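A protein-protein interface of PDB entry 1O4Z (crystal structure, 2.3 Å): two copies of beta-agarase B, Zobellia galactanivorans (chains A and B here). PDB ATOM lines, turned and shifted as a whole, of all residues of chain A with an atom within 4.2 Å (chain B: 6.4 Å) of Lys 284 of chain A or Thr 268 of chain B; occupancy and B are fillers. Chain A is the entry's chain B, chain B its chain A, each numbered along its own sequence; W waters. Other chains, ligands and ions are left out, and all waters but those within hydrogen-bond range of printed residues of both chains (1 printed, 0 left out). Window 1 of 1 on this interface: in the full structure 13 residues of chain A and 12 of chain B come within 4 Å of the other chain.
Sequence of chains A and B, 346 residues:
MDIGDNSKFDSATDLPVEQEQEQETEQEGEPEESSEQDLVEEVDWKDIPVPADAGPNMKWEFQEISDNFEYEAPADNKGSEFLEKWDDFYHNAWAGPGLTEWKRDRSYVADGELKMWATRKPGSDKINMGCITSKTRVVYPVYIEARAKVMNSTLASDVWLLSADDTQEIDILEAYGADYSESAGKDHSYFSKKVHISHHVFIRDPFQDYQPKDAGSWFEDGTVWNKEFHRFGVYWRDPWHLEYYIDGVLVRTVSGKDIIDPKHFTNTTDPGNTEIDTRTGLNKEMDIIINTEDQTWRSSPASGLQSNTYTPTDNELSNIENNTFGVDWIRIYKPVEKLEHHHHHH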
ATOM      1  N   SER A 163      18.487 -10.110 -30.047  1.00  0.00           N
ATOM      2  CA  SER A 163      17.986  -8.743 -29.973  1.00  0.00           C
ATOM      3  C   SER A 163      17.052  -8.430 -31.144  1.00  0.00           C
ATOM      4  O   SER A 163      17.138  -9.055 -32.208  1.00  0.00           O
ATOM      5  CB  SER A 163      19.146  -7.733 -29.892  1.00  0.00           C
ATOM      6  OG  SER A 163      19.923  -7.650 -31.077  1.00  0.00           O
ATOM      7  N   ASP A 165      16.862  -6.001 -33.185  1.00  0.00           N
ATOM      8  CA  ASP A 165      17.573  -5.504 -34.368  1.00  0.00           C
ATOM      9  C   ASP A 165      18.614  -6.489 -34.932  1.00  0.00           C
ATOM     10  O   ASP A 165      19.382  -6.141 -35.841  1.00  0.00           O
ATOM     11  CB  ASP A 165      18.246  -4.160 -34.034  1.00  0.00           C
ATOM     12  CG  ASP A 165      19.482  -4.297 -33.096  1.00  0.00           C
ATOM     13  OD1 ASP A 165      19.833  -5.411 -32.640  1.00  0.00           O
ATOM     14  OD2 ASP A 165      20.168  -3.319 -32.738  1.00  0.00           O
ATOM     15  N   THR A 167      21.451  -7.684 -33.941  1.00  0.00           N
ATOM     16  CA  THR A 167      22.886  -7.406 -33.794  1.00  0.00           C
ATOM     17  C   THR A 167      23.562  -8.174 -32.660  1.00  0.00           C
ATOM     18  O   THR A 167      24.787  -8.215 -32.597  1.00  0.00           O
ATOM     19  CB  THR A 167      23.178  -5.899 -33.541  1.00  0.00           C
ATOM     20  OG1 THR A 167      22.420  -5.434 -32.416  1.00  0.00           O
ATOM     21  CG2 THR A 167      22.747  -5.037 -34.711  1.00  0.00           C
ATOM     22  N   GLN A 168      22.776  -8.706 -31.738  1.00  0.00           N
ATOM     23  CA  GLN A 168      23.294  -9.343 -30.529  1.00  0.00           C
ATOM     24  C   GLN A 168      22.542 -10.650 -30.236  1.00  0.00           C
ATOM     25  O   GLN A 168      21.323 -10.692 -30.303  1.00  0.00           O
ATOM     26  CB  GLN A 168      23.165  -8.399 -29.339  1.00  0.00           C
ATOM     27  CG  GLN A 168      24.066  -7.217 -29.438  1.00  0.00           C
ATOM     28  CD  GLN A 168      23.906  -6.217 -28.296  1.00  0.00           C
ATOM     29  OE1 GLN A 168      24.383  -5.084 -28.406  1.00  0.00           O
ATOM     30  NE2 GLN A 168      23.242  -6.622 -27.215  1.00  0.00           N
ATOM     31  N   TRP A 236      23.378 -14.403 -17.850  1.00  0.00           N
ATOM     32  CA  TRP A 236      23.703 -13.159 -18.519  1.00  0.00           C
ATOM     33  C   TRP A 236      23.729 -12.065 -17.441  1.00  0.00           C
ATOM     34  O   TRP A 236      22.722 -11.449 -17.132  1.00  0.00           O
ATOM     35  CB  TRP A 236      22.634 -12.941 -19.568  1.00  0.00           C
ATOM     36  CG  TRP A 236      22.728 -11.724 -20.380  1.00  0.00           C
ATOM     37  CD1 TRP A 236      23.798 -10.886 -20.537  1.00  0.00           C
ATOM     38  CD2 TRP A 236      21.693 -11.217 -21.213  1.00  0.00           C
ATOM     39  NE1 TRP A 236      23.472  -9.866 -21.402  1.00  0.00           N
ATOM     40  CE2 TRP A 236      22.180 -10.044 -21.828  1.00  0.00           C
ATOM     41  CE3 TRP A 236      20.384 -11.625 -21.487  1.00  0.00           C
ATOM     42  CZ2 TRP A 236      21.401  -9.280 -22.699  1.00  0.00           C
ATOM     43  CZ3 TRP A 236      19.614 -10.864 -22.336  1.00  0.00           C
ATOM     44  CH2 TRP A 236      20.124  -9.707 -22.941  1.00  0.00           C
ATOM     45  N   LEU A 282      26.913  -6.792 -24.779  1.00  0.00           N
ATOM     46  CA  LEU A 282      25.608  -7.412 -24.889  1.00  0.00           C
ATOM     47  C   LEU A 282      24.636  -6.686 -23.946  1.00  0.00           C
ATOM     48  O   LEU A 282      24.335  -7.133 -22.848  1.00  0.00           O
ATOM     49  CB  LEU A 282      25.704  -8.899 -24.552  1.00  0.00           C
ATOM     50  CG  LEU A 282      26.646  -9.751 -25.399  1.00  0.00           C
ATOM     51  CD1 LEU A 282      26.801 -11.152 -24.773  1.00  0.00           C
ATOM     52  CD2 LEU A 282      26.133  -9.856 -26.827  1.00  0.00           C
ATOM     53  N   ASN A 283      24.154  -5.545 -24.402  1.00  0.00           N
ATOM     54  CA  ASN A 283      23.329  -4.679 -23.592  1.00  0.00           C
ATOM     55  C   ASN A 283      21.840  -4.729 -23.974  1.00  0.00           C
ATOM     56  O   ASN A 283      20.982  -4.398 -23.176  1.00  0.00           O
ATOM     57  CB  ASN A 283      23.845  -3.265 -23.742  1.00  0.00           C
ATOM     58  CG  ASN A 283      23.515  -2.670 -25.095  1.00  0.00           C
ATOM     59  OD1 ASN A 283      24.027  -3.122 -26.135  1.00  0.00           O
ATOM     60  ND2 ASN A 283      22.652  -1.647 -25.099  1.00  0.00           N
ATOM     61  N   LYS A 284      21.536  -5.157 -25.188  1.00  0.00           N
ATOM     62  CA  LYS A 284      20.184  -5.011 -25.740  1.00  0.00           C
ATOM     63  C   LYS A 284      19.291  -6.125 -25.249  1.00  0.00           C
ATOM     64  O   LYS A 284      19.713  -7.282 -25.214  1.00  0.00           O
ATOM     65  CB  LYS A 284      20.231  -5.046 -27.272  1.00  0.00           C
ATOM     66  CG  LYS A 284      20.817  -3.795 -27.884  1.00  0.00           C
ATOM     67  CD  LYS A 284      21.150  -3.928 -29.370  1.00  0.00           C
ATOM     68  CE  LYS A 284      22.129  -2.822 -29.809  1.00  0.00           C
ATOM     69  NZ  LYS A 284      22.446  -2.810 -31.265  1.00  0.00           N
ATOM     70  N   GLU A 285      18.060  -5.785 -24.877  1.00  0.00           N
ATOM     71  CA  GLU A 285      17.065  -6.786 -24.494  1.00  0.00           C
ATOM     72  C   GLU A 285      16.842  -7.765 -25.659  1.00  0.00           C
ATOM     73  O   GLU A 285      17.028  -7.420 -26.827  1.00  0.00           O
ATOM     74  CB  GLU A 285      15.758  -6.146 -24.041  1.00  0.00           C
ATOM     75  CG  GLU A 285      14.939  -5.497 -25.154  1.00  0.00           C
ATOM     76  CD  GLU A 285      13.681  -4.847 -24.620  1.00  0.00           C
ATOM     77  OE1 GLU A 285      13.412  -4.972 -23.412  1.00  0.00           O
ATOM     78  OE2 GLU A 285      12.957  -4.206 -25.409  1.00  0.00           O
ATOM     79  N   MET A 286      16.466  -8.989 -25.325  1.00  0.00           N
ATOM     80  CA  MET A 286      16.423 -10.067 -26.320  1.00  0.00           C
ATOM     81  C   MET A 286      15.155 -10.929 -26.251  1.00  0.00           C
ATOM     82  O   MET A 286      14.571 -11.139 -25.185  1.00  0.00           O
ATOM     83  CB  MET A 286      17.663 -10.968 -26.212  1.00  0.00           C
ATOM     84  CG  MET A 286      18.983 -10.270 -26.480  1.00  0.00           C
ATOM     85  SD  MET A 286      20.388 -11.405 -26.306  1.00  0.00           S
ATOM     86  CE  MET A 286      21.786 -10.281 -26.428  1.00  0.00           C
ATOM     87  N   PHE B 265      17.484   7.365 -21.827  1.00  0.00           N
ATOM     88  CA  PHE B 265      18.159   8.282 -22.760  1.00  0.00           C
ATOM     89  C   PHE B 265      19.339   7.628 -23.478  1.00  0.00           C
ATOM     90  O   PHE B 265      19.757   8.085 -24.544  1.00  0.00           O
ATOM     91  CB  PHE B 265      18.657   9.540 -22.018  1.00  0.00           C
ATOM     92  CG  PHE B 265      17.578  10.553 -21.695  1.00  0.00           C
ATOM     93  CD1 PHE B 265      16.237  10.321 -21.971  1.00  0.00           C
ATOM     94  CD2 PHE B 265      17.928  11.760 -21.098  1.00  0.00           C
ATOM     95  CE1 PHE B 265      15.268  11.275 -21.655  1.00  0.00           C
ATOM     96  CE2 PHE B 265      16.968  12.715 -20.776  1.00  0.00           C
ATOM     97  CZ  PHE B 265      15.640  12.474 -21.060  1.00  0.00           C
ATOM     98  N   THR B 266      19.876   6.559 -22.897  1.00  0.00           N
ATOM     99  CA  THR B 266      20.992   5.831 -23.528  1.00  0.00           C
ATOM    100  C   THR B 266      20.570   4.641 -24.418  1.00  0.00           C
ATOM    101  O   THR B 266      21.435   3.855 -24.819  1.00  0.00           O
ATOM    102  CB  THR B 266      22.000   5.341 -22.456  1.00  0.00           C
ATOM    103  OG1 THR B 266      21.386   4.370 -21.591  1.00  0.00           O
ATOM    104  CG2 THR B 266      22.449   6.491 -21.530  1.00  0.00           C
ATOM    105  N   ASN B 267      19.275   4.491 -24.718  1.00  0.00           N
ATOM    106  CA  ASN B 267      18.827   3.473 -25.700  1.00  0.00           C
ATOM    107  C   ASN B 267      19.574   3.676 -27.012  1.00  0.00           C
ATOM    108  O   ASN B 267      19.630   4.784 -27.508  1.00  0.00           O
ATOM    109  CB  ASN B 267      17.332   3.610 -26.039  1.00  0.00           C
ATOM    110  CG  ASN B 267      16.405   2.849 -25.096  1.00  0.00           C
ATOM    111  OD1 ASN B 267      16.838   2.172 -24.173  1.00  0.00           O
ATOM    112  ND2 ASN B 267      15.096   2.990 -25.328  1.00  0.00           N
ATOM    113  N   THR B 268      20.136   2.612 -27.573  1.00  0.00           N
ATOM    114  CA  THR B 268      20.727   2.643 -28.917  1.00  0.00           C
ATOM    115  C   THR B 268      19.642   2.819 -29.966  1.00  0.00           C
ATOM    116  O   THR B 268      19.901   3.343 -31.040  1.00  0.00           O
ATOM    117  CB  THR B 268      21.492   1.334 -29.240  1.00  0.00           C
ATOM    118  OG1 THR B 268      20.665   0.196 -28.967  1.00  0.00           O
ATOM    119  CG2 THR B 268      22.700   1.130 -28.322  1.00  0.00           C
ATOM    120  N   THR B 269      18.437   2.365 -29.659  1.00  0.00           N
ATOM    121  CA  THR B 269      17.298   2.567 -30.549  1.00  0.00           C
ATOM    122  C   THR B 269      16.158   3.294 -29.799  1.00  0.00           C
ATOM    123  O   THR B 269      15.669   2.839 -28.753  1.00  0.00           O
ATOM    124  CB  THR B 269      16.846   1.216 -31.198  1.00  0.00           C
ATOM    125  OG1 THR B 269      15.689   1.419 -32.032  1.00  0.00           O
ATOM    126  CG2 THR B 269      16.344   0.264 -30.183  1.00  0.00           C
ATOM    127  N   ASP B 270      15.798   4.463 -30.332  1.00  0.00           N
ATOM    128  CA  ASP B 270      14.706   5.305 -29.831  1.00  0.00           C
ATOM    129  C   ASP B 270      14.924   5.813 -28.382  1.00  0.00           C
ATOM    130  O   ASP B 270      14.283   5.349 -27.428  1.00  0.00           O
ATOM    131  CB  ASP B 270      13.374   4.572 -29.996  1.00  0.00           C
ATOM    132  CG  ASP B 270      12.168   5.483 -29.808  1.00  0.00           C
ATOM    133  OD1 ASP B 270      12.340   6.720 -29.689  1.00  0.00           O
ATOM    134  OD2 ASP B 270      11.006   5.032 -29.752  1.00  0.00           O
ATOM    135  N   PRO B 271      15.825   6.774 -28.223  1.00  0.00           N
ATOM    136  CA  PRO B 271      16.139   7.307 -26.886  1.00  0.00           C
ATOM    137  C   PRO B 271      14.930   7.963 -26.221  1.00  0.00           C
ATOM    138  O   PRO B 271      14.190   8.685 -26.900  1.00  0.00           O
ATOM    139  CB  PRO B 271      17.242   8.343 -27.165  1.00  0.00           C
ATOM    140  CG  PRO B 271      17.809   7.960 -28.520  1.00  0.00           C
ATOM    141  CD  PRO B 271      16.620   7.421 -29.288  1.00  0.00           C
ATOM    142  N   ASP B 277      13.996  -1.417 -24.079  1.00  0.00           N
ATOM    143  CA  ASP B 277      15.255  -1.370 -23.337  1.00  0.00           C
ATOM    144  C   ASP B 277      16.455  -1.846 -24.138  1.00  0.00           C
ATOM    145  O   ASP B 277      16.750  -3.041 -24.189  1.00  0.00           O
ATOM    146  CB  ASP B 277      15.161  -2.154 -22.023  1.00  0.00           C
ATOM    147  CG  ASP B 277      16.251  -1.761 -21.032  1.00  0.00           C
ATOM    148  OD1 ASP B 277      17.128  -0.945 -21.401  1.00  0.00           O
ATOM    149  OD2 ASP B 277      16.321  -2.224 -19.868  1.00  0.00           O
ATOM    150  N   THR B 278      17.141  -0.890 -24.761  1.00  0.00           N
ATOM    151  CA  THR B 278      18.438  -1.114 -25.360  1.00  0.00           C
ATOM    152  C   THR B 278      19.439  -0.178 -24.692  1.00  0.00           C
ATOM    153  O   THR B 278      20.354   0.355 -25.335  1.00  0.00           O
ATOM    154  CB  THR B 278      18.379  -0.811 -26.844  1.00  0.00           C
ATOM    155  OG1 THR B 278      17.709   0.441 -27.039  1.00  0.00           O
ATOM    156  CG2 THR B 278      17.524  -1.843 -27.592  1.00  0.00           C
ATOM    157  N   ARG B 279      19.263   0.032 -23.395  1.00  0.00           N
ATOM    158  CA  ARG B 279      20.080   1.005 -22.710  1.00  0.00           C
ATOM    159  C   ARG B 279      21.546   0.602 -22.676  1.00  0.00           C
ATOM    160  O   ARG B 279      21.929  -0.553 -22.516  1.00  0.00           O
ATOM    161  CB  ARG B 279      19.598   1.263 -21.293  1.00  0.00           C
ATOM    162  CG  ARG B 279      18.482   2.246 -21.188  1.00  0.00           C
ATOM    163  CD  ARG B 279      17.990   2.384 -19.774  1.00  0.00           C
ATOM    164  NE  ARG B 279      17.353   1.157 -19.311  1.00  0.00           N
ATOM    165  CZ  ARG B 279      16.732   1.017 -18.149  1.00  0.00           C
ATOM    166  NH1 ARG B 279      16.621   2.028 -17.311  1.00  0.00           N
ATOM    167  NH2 ARG B 279      16.184  -0.138 -17.836  1.00  0.00           N
ATOM    168  N   THR B 280      22.352   1.624 -22.761  1.00  0.00           N
ATOM    169  CA  THR B 280      23.782   1.512 -22.876  1.00  0.00           C
ATOM    170  C   THR B 280      24.469   1.813 -21.505  1.00  0.00           C
ATOM    171  O   THR B 280      25.508   1.221 -21.154  1.00  0.00           O
ATOM    172  CB  THR B 280      24.100   2.477 -23.999  1.00  0.00           C
ATOM    173  OG1 THR B 280      24.593   1.764 -25.148  1.00  0.00           O
ATOM    174  CG2 THR B 280      25.073   3.534 -23.626  1.00  0.00           C
HETATM  175  O   HOH W   1      20.804  -2.586 -21.264  1.00  0.00           O
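O of Asp 277 of chain B lies within hydrogen-bond range of N of Glu 285 of chain A, 3.1 Å away. O of Thr 278 of chain B sits at hydrogen-bond distance from ND2 of Asn 283 of chain A, 3.1 Å away. The backbone carbonyl oxygen of Arg 279 of chain B lies within hydrogen-bond range of the side-chain amide nitrogen of Asn 283 of chain A (2.9 Å).
Of the printed residues of chain B, Asn 283 of chain A touches Thr 278 (3.1 Å), Arg 279 (2.9 Å) and Thr 280 (3.9 Å). Printed residues of chain B within 4 Å of Glu 285 of chain A: Asp 277 (3.1 Å). Of the printed residues of chain A, Thr 268 of chain B touches Lys 284 (3.5 Å). Pro 271 of chain B touches none of the printed residues of chain A. Printed residues of chain A within 4 Å of Asp 277 of chain B: Glu 285. Printed residues of chain A within 4 Å of Thr 278 of chain B: Asn 283 (3.1 Å) and Lys 284 (3.8 Å). The nearest residue of chain B that does not touch Lys 284 of chain A is Asp 277 of chain B (4.1 Å).
Water W1 lies within hydrogen-bond range of O of Arg 279 of chain B and O of Asn 283 of chain A.
OD1 of Asn 267 of chain B sits at hydrogen-bond distance from N of Thr 278 of chain B (3.1 Å). The backbone NH (N) of Thr 268 of chain B lies within hydrogen-bond range of the backbone carbonyl oxygen (O) of Thr 278 of chain B (3.2 Å). The backbone NH (N) of Thr 269 of chain B is in hydrogen-bond range of the side-chain hydroxyl (OG1) of Thr 278 of chain B (3.3 Å). The side-chain carboxylate of Asp 277 of chain B is in salt-bridge range of the guanidinium group of Arg 279 of chain B, 2.9 Å away. The side-chain amino group (NZ) of Lys 284 of chain A sits at hydrogen-bond distance from the side-chain hydroxyl (OG1) of Thr 167 of chain A, 2.9 Å away. OD1 of Asn 283 of chain A lies close to OE1 of Gln 168 of chain A (3.0 Å).
No position is printed for both chains. Of the 6 pairs that touch across the chains among the printed residues, none has its exchanged pair printed and touching as well.
OG1 of Thr 280 of chain B touches ND2 of Asn 283 of chain A (3.9 Å). Lys 284 of chain A touches Thr 268 of chain B. CG2 of Thr 278 of chain B touches CG of Lys 284 of chain A, 3.8 Å away.
Of the 11 printed residues of chain B, 5 touch a printed residue of chain A. Of the 10 printed residues of chain A, 3 touch a printed residue of chain B. Among the printed residues, 6 pairs touch across the chains. Among the printed residues, no Asp or Glu carboxylate lies within 4 Å of a Lys or Arg side-chain nitrogen of the other chain.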
